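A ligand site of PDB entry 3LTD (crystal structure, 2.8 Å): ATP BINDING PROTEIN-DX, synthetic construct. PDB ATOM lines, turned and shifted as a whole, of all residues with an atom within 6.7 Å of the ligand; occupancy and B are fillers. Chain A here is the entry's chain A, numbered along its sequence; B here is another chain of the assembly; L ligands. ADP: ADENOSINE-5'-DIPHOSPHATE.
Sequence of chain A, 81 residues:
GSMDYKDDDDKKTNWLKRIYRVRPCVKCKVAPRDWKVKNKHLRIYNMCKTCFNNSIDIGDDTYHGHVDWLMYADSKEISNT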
ATOM      1  N   ARG A  33     -19.173   2.273  15.776  1.00  0.00           N
ATOM      2  CA  ARG A  33     -20.325   2.852  15.089  1.00  0.00           C
ATOM      3  C   ARG A  33     -21.607   2.801  15.887  1.00  0.00           C
ATOM      4  O   ARG A  33     -21.831   1.901  16.716  1.00  0.00           O
ATOM      5  CB  ARG A  33     -20.511   2.139  13.764  1.00  0.00           C
ATOM      6  CG  ARG A  33     -19.288   2.239  12.879  1.00  0.00           C
ATOM      7  CD  ARG A  33     -19.563   1.610  11.539  1.00  0.00           C
ATOM      8  NE  ARG A  33     -18.350   1.561  10.730  1.00  0.00           N
ATOM      9  CZ  ARG A  33     -18.324   1.183   9.448  1.00  0.00           C
ATOM     10  NH1 ARG A  33     -19.446   0.814   8.829  1.00  0.00           N
ATOM     11  NH2 ARG A  33     -17.176   1.167   8.793  1.00  0.00           N
ATOM     12  N   ASP A  34     -22.487   3.755  15.628  1.00  0.00           N
ATOM     13  CA  ASP A  34     -23.852   3.642  16.132  1.00  0.00           C
ATOM     14  C   ASP A  34     -24.517   2.466  15.427  1.00  0.00           C
ATOM     15  O   ASP A  34     -24.079   2.042  14.361  1.00  0.00           O
ATOM     16  CB  ASP A  34     -24.607   4.943  15.889  1.00  0.00           C
ATOM     17  CG  ASP A  34     -25.912   5.020  16.698  1.00  0.00           C
ATOM     18  OD1 ASP A  34     -26.030   4.338  17.739  1.00  0.00           O
ATOM     19  OD2 ASP A  34     -26.816   5.783  16.283  1.00  0.00           O
ATOM     20  N   TRP A  35     -25.562   1.925  16.042  1.00  0.00           N
ATOM     21  CA  TRP A  35     -26.297   0.789  15.527  1.00  0.00           C
ATOM     22  C   TRP A  35     -27.646   0.788  16.235  1.00  0.00           C
ATOM     23  O   TRP A  35     -27.827   1.456  17.259  1.00  0.00           O
ATOM     24  CB  TRP A  35     -25.564  -0.513  15.838  1.00  0.00           C
ATOM     25  CG  TRP A  35     -25.312  -0.643  17.316  1.00  0.00           C
ATOM     26  CD1 TRP A  35     -24.255  -0.098  18.020  1.00  0.00           C
ATOM     27  CD2 TRP A  35     -26.129  -1.304  18.289  1.00  0.00           C
ATOM     28  NE1 TRP A  35     -24.375  -0.394  19.359  1.00  0.00           N
ATOM     29  CE2 TRP A  35     -25.512  -1.130  19.556  1.00  0.00           C
ATOM     30  CE3 TRP A  35     -27.315  -2.039  18.221  1.00  0.00           C
ATOM     31  CZ2 TRP A  35     -26.048  -1.670  20.726  1.00  0.00           C
ATOM     32  CZ3 TRP A  35     -27.842  -2.572  19.399  1.00  0.00           C
ATOM     33  CH2 TRP A  35     -27.209  -2.383  20.626  1.00  0.00           C
ATOM     34  N   LYS A  36     -28.586   0.031  15.705  1.00  0.00           N
ATOM     35  CA  LYS A  36     -29.866  -0.223  16.379  1.00  0.00           C
ATOM     36  C   LYS A  36     -30.437  -1.527  15.859  1.00  0.00           C
ATOM     37  O   LYS A  36     -30.131  -1.924  14.730  1.00  0.00           O
ATOM     38  CB  LYS A  36     -30.866   0.926  16.160  1.00  0.00           C
ATOM     39  CG  LYS A  36     -31.630   0.829  14.863  1.00  0.00           C
ATOM     40  CD  LYS A  36     -32.637   1.950  14.685  1.00  0.00           C
ATOM     41  CE  LYS A  36     -33.496   1.688  13.421  1.00  0.00           C
ATOM     42  NZ  LYS A  36     -34.473   2.783  13.061  1.00  0.00           N
ATOM     43  N   LYS A  38     -33.574  -3.895  14.540  1.00  0.00           N
ATOM     44  CA  LYS A  38     -34.833  -3.614  13.848  1.00  0.00           C
ATOM     45  C   LYS A  38     -35.492  -4.855  13.236  1.00  0.00           C
ATOM     46  O   LYS A  38     -35.002  -5.406  12.235  1.00  0.00           O
ATOM     47  CB  LYS A  38     -34.612  -2.563  12.770  1.00  0.00           C
ATOM     48  CG  LYS A  38     -33.911  -3.060  11.523  1.00  0.00           C
ATOM     49  CD  LYS A  38     -34.470  -2.308  10.339  1.00  0.00           C
ATOM     50  CE  LYS A  38     -34.766  -0.858  10.765  1.00  0.00           C
ATOM     51  NZ  LYS A  38     -35.888  -0.292   9.954  1.00  0.00           N
ATOM     52  N   ARG A  43     -28.774  -3.167  12.277  1.00  0.00           N
ATOM     53  CA  ARG A  43     -28.351  -2.038  11.454  1.00  0.00           C
ATOM     54  C   ARG A  43     -27.092  -1.363  12.019  1.00  0.00           C
ATOM     55  O   ARG A  43     -27.119  -0.771  13.102  1.00  0.00           O
ATOM     56  CB  ARG A  43     -29.479  -1.004  11.342  1.00  0.00           C
ATOM     57  CG  ARG A  43     -29.046   0.315  10.701  1.00  0.00           C
ATOM     58  CD  ARG A  43     -30.212   1.147  10.144  1.00  0.00           C
ATOM     59  NE  ARG A  43     -31.007   0.346   9.214  1.00  0.00           N
ATOM     60  CZ  ARG A  43     -32.196   0.711   8.706  1.00  0.00           C
ATOM     61  NH1 ARG A  43     -32.722   1.890   9.006  1.00  0.00           N
ATOM     62  NH2 ARG A  43     -32.844  -0.104   7.871  1.00  0.00           N
ATOM     63  N   TYR A  45     -24.725   1.661  11.518  1.00  0.00           N
ATOM     64  CA  TYR A  45     -24.573   2.934  10.861  1.00  0.00           C
ATOM     65  C   TYR A  45     -23.115   3.146  10.530  1.00  0.00           C
ATOM     66  O   TYR A  45     -22.212   2.522  11.133  1.00  0.00           O
ATOM     67  CB  TYR A  45     -25.006   4.032  11.784  1.00  0.00           C
ATOM     68  CG  TYR A  45     -26.467   3.969  12.123  1.00  0.00           C
ATOM     69  CD1 TYR A  45     -27.438   4.185  11.147  1.00  0.00           C
ATOM     70  CD2 TYR A  45     -26.885   3.713  13.429  1.00  0.00           C
ATOM     71  CE1 TYR A  45     -28.781   4.123  11.448  1.00  0.00           C
ATOM     72  CE2 TYR A  45     -28.230   3.644  13.737  1.00  0.00           C
ATOM     73  CZ  TYR A  45     -29.167   3.853  12.744  1.00  0.00           C
ATOM     74  OH  TYR A  45     -30.500   3.785  13.039  1.00  0.00           O
ATOM     75  N   ASN A  46     -22.860   4.041   9.570  1.00  0.00           N
ATOM     76  CA  ASN A  46     -21.484   4.329   9.177  1.00  0.00           C
ATOM     77  C   ASN A  46     -20.654   5.109  10.205  1.00  0.00           C
ATOM     78  O   ASN A  46     -19.432   4.975  10.234  1.00  0.00           O
ATOM     79  CB  ASN A  46     -21.484   5.013   7.802  1.00  0.00           C
ATOM     80  CG  ASN A  46     -22.242   4.199   6.763  1.00  0.00           C
ATOM     81  OD1 ASN A  46     -22.165   2.969   6.748  1.00  0.00           O
ATOM     82  ND2 ASN A  46     -22.970   4.883   5.888  1.00  0.00           N
ATOM     83  N   MET A  47     -21.305   5.907  11.062  1.00  0.00           N
ATOM     84  CA  MET A  47     -20.593   6.721  12.064  1.00  0.00           C
ATOM     85  C   MET A  47     -20.965   6.442  13.527  1.00  0.00           C
ATOM     86  O   MET A  47     -22.023   5.896  13.847  1.00  0.00           O
ATOM     87  CB  MET A  47     -20.819   8.198  11.793  1.00  0.00           C
ATOM     88  CG  MET A  47     -20.334   8.661  10.436  1.00  0.00           C
ATOM     89  SD  MET A  47     -20.507  10.450  10.133  1.00  0.00           S
ATOM     90  CE  MET A  47     -22.167  10.641   9.476  1.00  0.00           C
ATOM     91  N   CYS A  48     -20.081   6.841  14.432  1.00  0.00           N
ATOM     92  CA  CYS A  48     -20.507   6.924  15.825  1.00  0.00           C
ATOM     93  C   CYS A  48     -21.565   8.055  15.969  1.00  0.00           C
ATOM     94  O   CYS A  48     -21.819   8.824  15.034  1.00  0.00           O
ATOM     95  CB  CYS A  48     -19.325   7.093  16.782  1.00  0.00           C
ATOM     96  SG  CYS A  48     -18.494   8.611  16.550  1.00  0.00           S
ATOM     97  N   LYS A  49     -22.214   8.123  17.112  1.00  0.00           N
ATOM     98  CA  LYS A  49     -23.219   9.149  17.313  1.00  0.00           C
ATOM     99  C   LYS A  49     -22.542  10.529  17.292  1.00  0.00           C
ATOM    100  O   LYS A  49     -23.088  11.489  16.713  1.00  0.00           O
ATOM    101  CB  LYS A  49     -23.908   8.974  18.662  1.00  0.00           C
ATOM    102  CG  LYS A  49     -25.266   9.671  18.746  1.00  0.00           C
ATOM    103  CD  LYS A  49     -26.271   8.895  17.926  1.00  0.00           C
ATOM    104  CE  LYS A  49     -27.597   9.565  17.872  1.00  0.00           C
ATOM    105  NZ  LYS A  49     -28.328   8.872  16.789  1.00  0.00           N
ATOM    106  N   CYS A  51     -19.988  11.690  15.806  1.00  0.00           N
ATOM    107  CA  CYS A  51     -19.738  12.142  14.462  1.00  0.00           C
ATOM    108  C   CYS A  51     -21.015  12.402  13.688  1.00  0.00           C
ATOM    109  O   CYS A  51     -21.096  13.369  12.926  1.00  0.00           O
ATOM    110  CB  CYS A  51     -18.877  11.155  13.701  1.00  0.00           C
ATOM    111  SG  CYS A  51     -17.146  11.320  14.143  1.00  0.00           S
ATOM    112  N   PHE A  52     -22.007  11.547  13.872  1.00  0.00           N
ATOM    113  CA  PHE A  52     -23.248  11.722  13.131  1.00  0.00           C
ATOM    114  C   PHE A  52     -23.944  13.033  13.471  1.00  0.00           C
ATOM    115  O   PHE A  52     -24.354  13.792  12.561  1.00  0.00           O
ATOM    116  CB  PHE A  52     -24.189  10.584  13.392  1.00  0.00           C
ATOM    117  CG  PHE A  52     -25.519  10.785  12.767  1.00  0.00           C
ATOM    118  CD1 PHE A  52     -25.641  10.809  11.373  1.00  0.00           C
ATOM    119  CD2 PHE A  52     -26.648  10.991  13.548  1.00  0.00           C
ATOM    120  CE1 PHE A  52     -26.894  10.997  10.774  1.00  0.00           C
ATOM    121  CE2 PHE A  52     -27.903  11.200  12.956  1.00  0.00           C
ATOM    122  CZ  PHE A  52     -28.015  11.196  11.564  1.00  0.00           C
ATOM    123  N   ASN A  53     -24.082  13.325  14.762  1.00  0.00           N
ATOM    124  CA  ASN A  53     -24.704  14.587  15.148  1.00  0.00           C
ATOM    125  C   ASN A  53     -23.887  15.761  14.646  1.00  0.00           C
ATOM    126  O   ASN A  53     -24.428  16.804  14.284  1.00  0.00           O
ATOM    127  CB  ASN A  53     -24.866  14.693  16.663  1.00  0.00           C
ATOM    128  CG  ASN A  53     -25.858  13.672  17.239  1.00  0.00           C
ATOM    129  OD1 ASN A  53     -26.855  13.326  16.590  1.00  0.00           O
ATOM    130  ND2 ASN A  53     -25.580  13.177  18.446  1.00  0.00           N
ATOM    131  N   SER A  55     -22.001  15.821  11.897  1.00  0.00           N
ATOM    132  CA  SER A  55     -22.282  15.914  10.478  1.00  0.00           C
ATOM    133  C   SER A  55     -23.579  16.693  10.179  1.00  0.00           C
ATOM    134  O   SER A  55     -23.634  17.450   9.204  1.00  0.00           O
ATOM    135  CB  SER A  55     -22.340  14.511   9.860  1.00  0.00           C
ATOM    136  OG  SER A  55     -23.647  13.993   9.897  1.00  0.00           O
ATOM    137  N   TYR A  63     -21.143  10.996   4.752  1.00  0.00           N
ATOM    138  CA  TYR A  63     -21.014   9.684   5.425  1.00  0.00           C
ATOM    139  C   TYR A  63     -22.309   9.027   5.971  1.00  0.00           C
ATOM    140  O   TYR A  63     -22.256   7.990   6.599  1.00  0.00           O
ATOM    141  CB  TYR A  63     -19.940   9.716   6.499  1.00  0.00           C
ATOM    142  CG  TYR A  63     -18.679  10.182   5.867  1.00  0.00           C
ATOM    143  CD1 TYR A  63     -17.905   9.293   5.137  1.00  0.00           C
ATOM    144  CD2 TYR A  63     -18.288  11.516   5.929  1.00  0.00           C
ATOM    145  CE1 TYR A  63     -16.737   9.701   4.518  1.00  0.00           C
ATOM    146  CE2 TYR A  63     -17.108  11.953   5.298  1.00  0.00           C
ATOM    147  CZ  TYR A  63     -16.347  11.027   4.587  1.00  0.00           C
ATOM    148  OH  TYR A  63     -15.196  11.407   3.950  1.00  0.00           O
ATOM    149  N   HIS A  64     -23.441   9.652   5.725  1.00  0.00           N
ATOM    150  CA  HIS A  64     -24.706   9.089   6.141  1.00  0.00           C
ATOM    151  C   HIS A  64     -24.936   7.705   5.517  1.00  0.00           C
ATOM    152  O   HIS A  64     -24.503   7.437   4.409  1.00  0.00           O
ATOM    153  CB  HIS A  64     -25.816  10.090   5.795  1.00  0.00           C
ATOM    154  CG  HIS A  64     -25.753  11.314   6.648  1.00  0.00           C
ATOM    155  ND1 HIS A  64     -26.782  12.220   6.751  1.00  0.00           N
ATOM    156  CD2 HIS A  64     -24.779  11.757   7.495  1.00  0.00           C
ATOM    157  CE1 HIS A  64     -26.443  13.172   7.610  1.00  0.00           C
ATOM    158  NE2 HIS A  64     -25.238  12.914   8.071  1.00  0.00           N
ATOM    159  N   GLY A  65     -25.579   6.808   6.243  1.00  0.00           N
ATOM    160  CA  GLY A  65     -25.774   5.466   5.712  1.00  0.00           C
ATOM    161  C   GLY A  65     -25.612   4.356   6.743  1.00  0.00           C
ATOM    162  O   GLY A  65     -25.169   4.586   7.883  1.00  0.00           O
ATOM    163  N   HIS A  66     -25.971   3.139   6.344  1.00  0.00           N
ATOM    164  CA  HIS A  66     -25.914   1.980   7.207  1.00  0.00           C
ATOM    165  C   HIS A  66     -25.856   0.729   6.359  1.00  0.00           C
ATOM    166  O   HIS A  66     -26.182   0.763   5.162  1.00  0.00           O
ATOM    167  CB  HIS A  66     -27.175   1.929   8.066  1.00  0.00           C
ATOM    168  CG  HIS A  66     -28.426   2.027   7.273  1.00  0.00           C
ATOM    169  ND1 HIS A  66     -29.056   3.223   7.013  1.00  0.00           N
ATOM    170  CD2 HIS A  66     -29.154   1.076   6.631  1.00  0.00           C
ATOM    171  CE1 HIS A  66     -30.132   3.004   6.280  1.00  0.00           C
ATOM    172  NE2 HIS A  66     -30.210   1.711   6.033  1.00  0.00           N
ATOM    173  N   ASP B   8     -23.291   2.220  -0.041  1.00  0.00           N
ATOM    174  CA  ASP B   8     -23.547   1.260   1.054  1.00  0.00           C
ATOM    175  C   ASP B   8     -23.673  -0.216   0.611  1.00  0.00           C
ATOM    176  O   ASP B   8     -23.221  -1.114   1.325  1.00  0.00           O
ATOM    177  CB  ASP B   8     -24.787   1.677   1.877  1.00  0.00           C
ATOM    178  CG  ASP B   8     -24.491   2.804   2.867  1.00  0.00           C
ATOM    179  OD1 ASP B   8     -23.322   2.970   3.270  1.00  0.00           O
ATOM    180  OD2 ASP B   8     -25.448   3.518   3.230  1.00  0.00           O
HETATM  181  PB  ADP L   1     -35.680   5.104   9.427  1.00  0.00           P
HETATM  182  O1B ADP L   1     -36.082   4.175   8.265  1.00  0.00           O
HETATM  183  O2B ADP L   1     -36.136   6.570   9.269  1.00  0.00           O
HETATM  184  O3B ADP L   1     -35.964   4.481  10.807  1.00  0.00           O
HETATM  185  PA  ADP L   1     -33.018   5.637  10.415  1.00  0.00           P
HETATM  186  O1A ADP L   1     -32.191   4.392  10.714  1.00  0.00           O
HETATM  187  O2A ADP L   1     -33.728   6.439  11.513  1.00  0.00           O
HETATM  188  O3A ADP L   1     -34.062   5.238   9.242  1.00  0.00           O
HETATM  189  O5' ADP L   1     -31.971   6.603   9.633  1.00  0.00           O
HETATM  190  C5' ADP L   1     -32.353   7.632   8.716  1.00  0.00           C
HETATM  191  C4' ADP L   1     -31.112   8.063   7.959  1.00  0.00           C
HETATM  192  O4' ADP L   1     -30.165   8.541   8.909  1.00  0.00           O
HETATM  193  C3' ADP L   1     -30.415   6.925   7.220  1.00  0.00           C
HETATM  194  O3' ADP L   1     -29.834   7.451   6.015  1.00  0.00           O
HETATM  195  C2' ADP L   1     -29.282   6.549   8.142  1.00  0.00           C
HETATM  196  O2' ADP L   1     -28.149   5.988   7.486  1.00  0.00           O
HETATM  197  C1' ADP L   1     -28.916   7.907   8.672  1.00  0.00           C
HETATM  198  N9  ADP L   1     -28.163   7.785   9.930  1.00  0.00           N
HETATM  199  C8  ADP L   1     -28.695   7.762  11.170  1.00  0.00           C
HETATM  200  N7  ADP L   1     -27.719   7.631  12.104  1.00  0.00           N
HETATM  201  C5  ADP L   1     -26.550   7.559  11.452  1.00  0.00           C
HETATM  202  C6  ADP L   1     -25.154   7.424  11.852  1.00  0.00           C
HETATM  203  N6  ADP L   1     -24.846   7.332  13.161  1.00  0.00           N
HETATM  204  N1  ADP L   1     -24.229   7.408  10.876  1.00  0.00           N
HETATM  205  C2  ADP L   1     -24.556   7.507   9.557  1.00  0.00           C
HETATM  206  N3  ADP L   1     -25.814   7.615   9.121  1.00  0.00           N
HETATM  207  C4  ADP L   1     -26.829   7.652  10.020  1.00  0.00           C
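The backbone carbonyl oxygen (O) of Asp 34 is in hydrogen-bond range of the backbone NH (N) of Tyr 45. The backbone NH of His 66 is in hydrogen-bond range of the side-chain carboxylate of Asp 8 of chain B, at 3.2 Å. The backbone NH (N) of Asn 46 lies within hydrogen-bond range of the backbone carbonyl oxygen (O) of Gly 65 (2.9 Å). The backbone carbonyl oxygen (O) of Lys 36 lies within hydrogen-bond range of the backbone NH (N) of Arg 43, 3.1 Å away. The backbone carbonyl oxygen (O) of Phe 52 lies within hydrogen-bond range of the side-chain hydroxyl (OG) of Ser 55 (2.8 Å). NE2 of His 64 lies within hydrogen-bond range of OG of Ser 55 (2.7 Å). The side-chain amino group of Lys 49 is in salt-bridge range of the side-chain carboxylate of Asp 34. The side-chain amide nitrogen (ND2) of Asn 46 lies within hydrogen-bond range of the backbone carbonyl oxygen (O) of Tyr 63 (3.3 Å).
Residues that only touch the ligand: Asp 34, Asn 46, Cys 48, Phe 52, Tyr 63 and His 64. Hydrophobic or aromatic side chains that line the ligand: Tyr 45, Met 47, Phe 52 and His 66. Within 4 Å of the ligand: Asp 34, Lys 36, Arg 43, Tyr 45, Asn 46, Met 47, Cys 48, Phe 52, Tyr 63, His 64, Gly 65 and His 66. Along chain A the residues within 4 Å of the ligand span positions 34 to 66. The nearest printed residue that does not touch the ligand is Lys 38 (4.8 Å).
The side-chain hydroxyl of Tyr 45 sits at hydrogen-bond distance from an oxygen (O1A) of the ligand, at 2.9 Å. A ring nitrogen (ND1) of His 66 lies within hydrogen-bond range of an oxygen (O2') of the ligand (2.9 Å). N of Gly 65 is in hydrogen-bond range of O2' of the ligand. O2' of the ligand sits close to O of Gly 65 (3.3 Å). The guanidinium group (NH1) of Arg 43 lies within salt-bridge range of an oxygen (O1A) of the ligand, 3.1 Å away. An oxygen (O3B) of the ligand lies within salt-bridge range of the side-chain amino group of Lys 36 (3.2 Å). The backbone NH (N) of Met 47 is in hydrogen-bond range of a nitrogen (N1) of the ligand (3.3 Å). The backbone carbonyl oxygen (O) of Met 47 sits at hydrogen-bond distance from a nitrogen (N6) of the ligand.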
